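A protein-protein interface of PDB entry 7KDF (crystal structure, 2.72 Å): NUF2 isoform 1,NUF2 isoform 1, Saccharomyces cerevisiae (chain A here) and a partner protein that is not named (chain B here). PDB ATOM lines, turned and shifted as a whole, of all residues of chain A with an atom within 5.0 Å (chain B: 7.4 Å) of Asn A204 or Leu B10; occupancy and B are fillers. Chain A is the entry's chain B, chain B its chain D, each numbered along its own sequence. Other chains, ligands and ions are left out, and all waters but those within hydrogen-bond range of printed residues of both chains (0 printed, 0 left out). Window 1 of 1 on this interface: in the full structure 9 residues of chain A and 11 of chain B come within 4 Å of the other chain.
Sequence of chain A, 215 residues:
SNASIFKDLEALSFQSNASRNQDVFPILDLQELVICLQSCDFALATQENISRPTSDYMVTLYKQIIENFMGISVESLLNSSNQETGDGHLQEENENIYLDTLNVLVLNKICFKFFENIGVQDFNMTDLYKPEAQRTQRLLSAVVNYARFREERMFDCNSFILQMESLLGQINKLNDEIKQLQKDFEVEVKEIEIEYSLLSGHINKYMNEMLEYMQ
Phe B7 touches Tyr A196 (CA to OH, 3.3 Å).
Ser A200 touches Leu B10 (OG to CD1, 3.3 Å).
Asn A204 touches Leu B10 (OD1 to CD1, 3.6 Å).
Arg B13 touches Asn A204 (NE to ND2, 3.6 Å).
CE of Met A207 touches O of Arg B13, at 3.4 Å.
Met A207 touches Met B14 (CE to CA, 3.3 Å).
Among the printed residues, no Asp or Glu carboxylate lies within 4 Å of a Lys or Arg side-chain nitrogen of the other chain.
The backbone carbonyl oxygen (O) of Ser A200 lies close to the side-chain amide oxygen (OD1) of Asn A204 (3.0 Å).
The side-chain amide nitrogen (ND2) of Asn A208 lies within hydrogen-bond range of the backbone carbonyl oxygen (O) of Asn A204, at 2.9 Å.
Of the printed residues of chain B, Tyr A196 touches Phe B7.
Printed residues of chain B within 4 Å of Ser A200: Leu B10.
Of the printed residues of chain B, Met A207 touches Arg B13 (3.4 Å) and Met B14 (3.3 Å).
Of the printed residues of chain A, Phe B7 touches Tyr A196 (3.3 Å).
Of chain A, only Ser A200 and Asn A204 come within 4 Å of Leu B10.
Of the printed residues of chain A, Met B14 touches Met A207.
The nearest residue of chain A that does not touch Leu B10 is Ile A203 (4.2 Å).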
ATOM      1  N   TYR A 196      11.978  17.378 -26.058  1.00  0.00           N
ATOM      2  CA  TYR A 196      11.970  16.149 -25.273  1.00  0.00           C
ATOM      3  C   TYR A 196      11.943  14.923 -26.176  1.00  0.00           C
ATOM      4  O   TYR A 196      12.584  13.908 -25.875  1.00  0.00           O
ATOM      5  CB  TYR A 196      10.780  16.116 -24.317  1.00  0.00           C
ATOM      6  CG  TYR A 196      10.573  14.742 -23.723  1.00  0.00           C
ATOM      7  CD1 TYR A 196      11.268  14.346 -22.588  1.00  0.00           C
ATOM      8  CD2 TYR A 196       9.702  13.831 -24.311  1.00  0.00           C
ATOM      9  CE1 TYR A 196      11.095  13.085 -22.049  1.00  0.00           C
ATOM     10  CE2 TYR A 196       9.526  12.568 -23.782  1.00  0.00           C
ATOM     11  CZ  TYR A 196      10.223  12.200 -22.650  1.00  0.00           C
ATOM     12  OH  TYR A 196      10.040  10.942 -22.122  1.00  0.00           O
ATOM     13  N   SER A 200      14.318  11.816 -26.028  1.00  0.00           N
ATOM     14  CA  SER A 200      13.800  10.467 -25.822  1.00  0.00           C
ATOM     15  C   SER A 200      14.325   9.509 -26.883  1.00  0.00           C
ATOM     16  O   SER A 200      14.711   8.376 -26.571  1.00  0.00           O
ATOM     17  CB  SER A 200      12.273  10.477 -25.826  1.00  0.00           C
ATOM     18  OG  SER A 200      11.763   9.160 -25.695  1.00  0.00           O
ATOM     19  N   GLY A 201      14.340   9.946 -28.143  1.00  0.00           N
ATOM     20  CA  GLY A 201      14.915   9.120 -29.191  1.00  0.00           C
ATOM     21  C   GLY A 201      16.405   8.916 -29.008  1.00  0.00           C
ATOM     22  O   GLY A 201      16.933   7.836 -29.293  1.00  0.00           O
ATOM     23  N   HIS A 202      17.101   9.948 -28.524  1.00  0.00           N
ATOM     24  CA  HIS A 202      18.537   9.847 -28.283  1.00  0.00           C
ATOM     25  C   HIS A 202      18.855   8.790 -27.230  1.00  0.00           C
ATOM     26  O   HIS A 202      19.798   8.007 -27.394  1.00  0.00           O
ATOM     27  CB  HIS A 202      19.080  11.213 -27.861  1.00  0.00           C
ATOM     28  CG  HIS A 202      20.564  11.346 -27.987  1.00  0.00           C
ATOM     29  ND1 HIS A 202      21.183  11.704 -29.167  1.00  0.00           N
ATOM     30  CD2 HIS A 202      21.554  11.195 -27.076  1.00  0.00           C
ATOM     31  CE1 HIS A 202      22.489  11.754 -28.978  1.00  0.00           C
ATOM     32  NE2 HIS A 202      22.741  11.451 -27.717  1.00  0.00           N
ATOM     33  N   ILE A 203      18.086   8.756 -26.139  1.00  0.00           N
ATOM     34  CA  ILE A 203      18.337   7.782 -25.081  1.00  0.00           C
ATOM     35  C   ILE A 203      18.010   6.368 -25.552  1.00  0.00           C
ATOM     36  O   ILE A 203      18.748   5.419 -25.256  1.00  0.00           O
ATOM     37  CB  ILE A 203      17.545   8.161 -23.816  1.00  0.00           C
ATOM     38  CG1 ILE A 203      17.983   9.537 -23.304  1.00  0.00           C
ATOM     39  CG2 ILE A 203      17.705   7.100 -22.734  1.00  0.00           C
ATOM     40  CD1 ILE A 203      17.243   9.994 -22.065  1.00  0.00           C
ATOM     41  N   ASN A 204      16.890   6.202 -26.270  1.00  0.00           N
ATOM     42  CA  ASN A 204      16.569   4.906 -26.867  1.00  0.00           C
ATOM     43  C   ASN A 204      17.599   4.480 -27.899  1.00  0.00           C
ATOM     44  O   ASN A 204      17.965   3.302 -27.956  1.00  0.00           O
ATOM     45  CB  ASN A 204      15.164   4.929 -27.470  1.00  0.00           C
ATOM     46  CG  ASN A 204      14.076   4.787 -26.423  1.00  0.00           C
ATOM     47  OD1 ASN A 204      13.359   5.732 -26.099  1.00  0.00           O
ATOM     48  ND2 ASN A 204      13.864   3.543 -25.989  1.00  0.00           N
ATOM     49  N   LYS A 205      18.064   5.408 -28.736  1.00  0.00           N
ATOM     50  CA  LYS A 205      19.128   5.068 -29.674  1.00  0.00           C
ATOM     51  C   LYS A 205      20.367   4.585 -28.924  1.00  0.00           C
ATOM     52  O   LYS A 205      20.934   3.536 -29.251  1.00  0.00           O
ATOM     53  CB  LYS A 205      19.439   6.276 -30.559  1.00  0.00           C
ATOM     54  CG  LYS A 205      20.501   6.039 -31.629  1.00  0.00           C
ATOM     55  CD  LYS A 205      20.686   7.309 -32.449  1.00  0.00           C
ATOM     56  CE  LYS A 205      21.813   7.154 -33.466  1.00  0.00           C
ATOM     57  NZ  LYS A 205      21.929   8.442 -34.217  1.00  0.00           N
ATOM     58  N   TYR A 206      20.752   5.310 -27.868  1.00  0.00           N
ATOM     59  CA  TYR A 206      21.902   4.949 -27.037  1.00  0.00           C
ATOM     60  C   TYR A 206      21.794   3.531 -26.475  1.00  0.00           C
ATOM     61  O   TYR A 206      22.741   2.741 -26.562  1.00  0.00           O
ATOM     62  CB  TYR A 206      22.020   5.970 -25.905  1.00  0.00           C
ATOM     63  CG  TYR A 206      23.039   5.657 -24.841  1.00  0.00           C
ATOM     64  CD1 TYR A 206      24.397   5.779 -25.099  1.00  0.00           C
ATOM     65  CD2 TYR A 206      22.645   5.270 -23.568  1.00  0.00           C
ATOM     66  CE1 TYR A 206      25.335   5.509 -24.127  1.00  0.00           C
ATOM     67  CE2 TYR A 206      23.575   4.997 -22.589  1.00  0.00           C
ATOM     68  CZ  TYR A 206      24.921   5.116 -22.874  1.00  0.00           C
ATOM     69  OH  TYR A 206      25.857   4.842 -21.902  1.00  0.00           O
ATOM     70  N   MET A 207      20.649   3.194 -25.882  1.00  0.00           N
ATOM     71  CA  MET A 207      20.486   1.859 -25.315  1.00  0.00           C
ATOM     72  C   MET A 207      20.551   0.789 -26.397  1.00  0.00           C
ATOM     73  O   MET A 207      21.130  -0.281 -26.187  1.00  0.00           O
ATOM     74  CB  MET A 207      19.164   1.775 -24.558  1.00  0.00           C
ATOM     75  CG  MET A 207      19.157   2.567 -23.281  1.00  0.00           C
ATOM     76  SD  MET A 207      17.470   2.841 -22.728  1.00  0.00           S
ATOM     77  CE  MET A 207      17.701   2.711 -20.981  1.00  0.00           C
ATOM     78  N   ASN A 208      19.971   1.066 -27.567  1.00  0.00           N
ATOM     79  CA  ASN A 208      19.951   0.064 -28.628  1.00  0.00           C
ATOM     80  C   ASN A 208      21.362  -0.286 -29.087  1.00  0.00           C
ATOM     81  O   ASN A 208      21.682  -1.463 -29.286  1.00  0.00           O
ATOM     82  CB  ASN A 208      19.104   0.557 -29.801  1.00  0.00           C
ATOM     83  CG  ASN A 208      17.639   0.719 -29.435  1.00  0.00           C
ATOM     84  OD1 ASN A 208      17.130   0.041 -28.538  1.00  0.00           O
ATOM     85  ND2 ASN A 208      16.951   1.623 -30.128  1.00  0.00           N
ATOM     86  N   ALA B   6       4.914  10.871 -20.394  1.00  0.00           N
ATOM     87  CA  ALA B   6       5.240   9.453 -20.440  1.00  0.00           C
ATOM     88  C   ALA B   6       6.700   9.179 -20.093  1.00  0.00           C
ATOM     89  O   ALA B   6       7.203   8.088 -20.384  1.00  0.00           O
ATOM     90  CB  ALA B   6       4.911   8.884 -21.821  1.00  0.00           C
ATOM     91  N   PHE B   7       7.382  10.144 -19.474  1.00  0.00           N
ATOM     92  CA  PHE B   7       8.798   9.978 -19.165  1.00  0.00           C
ATOM     93  C   PHE B   7       9.039   8.847 -18.175  1.00  0.00           C
ATOM     94  O   PHE B   7      10.119   8.244 -18.175  1.00  0.00           O
ATOM     95  CB  PHE B   7       9.366  11.285 -18.620  1.00  0.00           C
ATOM     96  CG  PHE B   7      10.788  11.181 -18.172  1.00  0.00           C
ATOM     97  CD1 PHE B   7      11.798  10.910 -19.085  1.00  0.00           C
ATOM     98  CD2 PHE B   7      11.117  11.345 -16.838  1.00  0.00           C
ATOM     99  CE1 PHE B   7      13.109  10.814 -18.676  1.00  0.00           C
ATOM    100  CE2 PHE B   7      12.426  11.249 -16.423  1.00  0.00           C
ATOM    101  CZ  PHE B   7      13.423  10.984 -17.347  1.00  0.00           C
ATOM    102  N   SER B   8       8.058   8.545 -17.324  1.00  0.00           N
ATOM    103  CA  SER B   8       8.222   7.462 -16.363  1.00  0.00           C
ATOM    104  C   SER B   8       8.365   6.106 -17.040  1.00  0.00           C
ATOM    105  O   SER B   8       8.949   5.192 -16.448  1.00  0.00           O
ATOM    106  CB  SER B   8       7.041   7.441 -15.391  1.00  0.00           C
ATOM    107  OG  SER B   8       5.817   7.610 -16.084  1.00  0.00           O
ATOM    108  N   ASP B   9       7.848   5.952 -18.262  1.00  0.00           N
ATOM    109  CA  ASP B   9       8.044   4.707 -18.997  1.00  0.00           C
ATOM    110  C   ASP B   9       9.506   4.535 -19.390  1.00  0.00           C
ATOM    111  O   ASP B   9      10.099   3.471 -19.179  1.00  0.00           O
ATOM    112  CB  ASP B   9       7.149   4.686 -20.238  1.00  0.00           C
ATOM    113  CG  ASP B   9       5.675   4.573 -19.896  1.00  0.00           C
ATOM    114  OD1 ASP B   9       5.349   4.396 -18.703  1.00  0.00           O
ATOM    115  OD2 ASP B   9       4.842   4.665 -20.824  1.00  0.00           O
ATOM    116  N   LEU B  10      10.098   5.581 -19.969  1.00  0.00           N
ATOM    117  CA  LEU B  10      11.520   5.572 -20.287  1.00  0.00           C
ATOM    118  C   LEU B  10      12.390   5.558 -19.034  1.00  0.00           C
ATOM    119  O   LEU B  10      13.460   4.938 -19.035  1.00  0.00           O
ATOM    120  CB  LEU B  10      11.830   6.762 -21.200  1.00  0.00           C
ATOM    121  CG  LEU B  10      13.235   7.056 -21.711  1.00  0.00           C
ATOM    122  CD1 LEU B  10      13.210   7.642 -23.102  1.00  0.00           C
ATOM    123  CD2 LEU B  10      13.739   8.130 -20.787  1.00  0.00           C
ATOM    124  N   GLU B  11      11.950   6.213 -17.958  1.00  0.00           N
ATOM    125  CA  GLU B  11      12.691   6.144 -16.702  1.00  0.00           C
ATOM    126  C   GLU B  11      12.802   4.707 -16.212  1.00  0.00           C
ATOM    127  O   GLU B  11      13.853   4.295 -15.707  1.00  0.00           O
ATOM    128  CB  GLU B  11      12.020   7.027 -15.649  1.00  0.00           C
ATOM    129  CG  GLU B  11      12.629   6.924 -14.257  1.00  0.00           C
ATOM    130  CD  GLU B  11      12.239   8.092 -13.365  1.00  0.00           C
ATOM    131  OE1 GLU B  11      11.232   8.766 -13.672  1.00  0.00           O
ATOM    132  OE2 GLU B  11      12.947   8.348 -12.367  1.00  0.00           O
ATOM    133  N   ARG B  12      11.725   3.928 -16.346  1.00  0.00           N
ATOM    134  CA  ARG B  12      11.772   2.523 -15.954  1.00  0.00           C
ATOM    135  C   ARG B  12      12.771   1.746 -16.800  1.00  0.00           C
ATOM    136  O   ARG B  12      13.530   0.923 -16.275  1.00  0.00           O
ATOM    137  CB  ARG B  12      10.382   1.897 -16.066  1.00  0.00           C
ATOM    138  CG  ARG B  12       9.670   1.705 -14.736  1.00  0.00           C
ATOM    139  CD  ARG B  12       8.470   0.779 -14.884  1.00  0.00           C
ATOM    140  NE  ARG B  12       7.318   1.463 -15.469  1.00  0.00           N
ATOM    141  CZ  ARG B  12       6.986   1.402 -16.755  1.00  0.00           C
ATOM    142  NH1 ARG B  12       7.715   0.684 -17.600  1.00  0.00           N
ATOM    143  NH2 ARG B  12       5.921   2.058 -17.198  1.00  0.00           N
ATOM    144  N   ARG B  13      12.782   1.989 -18.113  1.00  0.00           N
ATOM    145  CA  ARG B  13      13.743   1.315 -18.981  1.00  0.00           C
ATOM    146  C   ARG B  13      15.171   1.692 -18.610  1.00  0.00           C
ATOM    147  O   ARG B  13      16.075   0.851 -18.652  1.00  0.00           O
ATOM    148  CB  ARG B  13      13.463   1.660 -20.443  1.00  0.00           C
ATOM    149  CG  ARG B  13      12.489   0.725 -21.137  1.00  0.00           C
ATOM    150  CD  ARG B  13      12.625   0.820 -22.650  1.00  0.00           C
ATOM    151  NE  ARG B  13      12.132   2.096 -23.160  1.00  0.00           N
ATOM    152  CZ  ARG B  13      10.877   2.316 -23.536  1.00  0.00           C
ATOM    153  NH1 ARG B  13       9.980   1.341 -23.462  1.00  0.00           N
ATOM    154  NH2 ARG B  13      10.515   3.511 -23.987  1.00  0.00           N
ATOM    155  N   MET B  14      15.388   2.957 -18.244  1.00  0.00           N
ATOM    156  CA  MET B  14      16.720   3.405 -17.858  1.00  0.00           C
ATOM    157  C   MET B  14      17.202   2.701 -16.598  1.00  0.00           C
ATOM    158  O   MET B  14      18.341   2.225 -16.541  1.00  0.00           O
ATOM    159  CB  MET B  14      16.726   4.919 -17.677  1.00  0.00           C
ATOM    160  CG  MET B  14      17.002   5.660 -18.961  1.00  0.00           C
ATOM    161  SD  MET B  14      16.288   7.301 -18.945  1.00  0.00           S
ATOM    162  CE  MET B  14      17.612   8.282 -18.264  1.00  0.00           C
ATOM    163  N   ASP B  15      16.347   2.619 -15.576  1.00  0.00           N
ATOM    164  CA  ASP B  15      16.721   1.916 -14.354  1.00  0.00           C
ATOM    165  C   ASP B  15      17.039   0.452 -14.633  1.00  0.00           C
ATOM    166  O   ASP B  15      17.919  -0.133 -13.991  1.00  0.00           O
ATOM    167  CB  ASP B  15      15.609   2.048 -13.313  1.00  0.00           C
ATOM    168  CG  ASP B  15      15.726   3.326 -12.501  1.00  0.00           C
ATOM    169  OD1 ASP B  15      16.702   3.449 -11.730  1.00  0.00           O
ATOM    170  OD2 ASP B  15      14.858   4.213 -12.648  1.00  0.00           O
ATOM    171  N   GLY B  16      16.335  -0.158 -15.588  1.00  0.00           N
ATOM    172  CA  GLY B  16      16.621  -1.545 -15.924  1.00  0.00           C
ATOM    173  C   GLY B  16      17.934  -1.707 -16.669  1.00  0.00           C
ATOM    174  O   GLY B  16      18.772  -2.536 -16.304  1.00  0.00           O
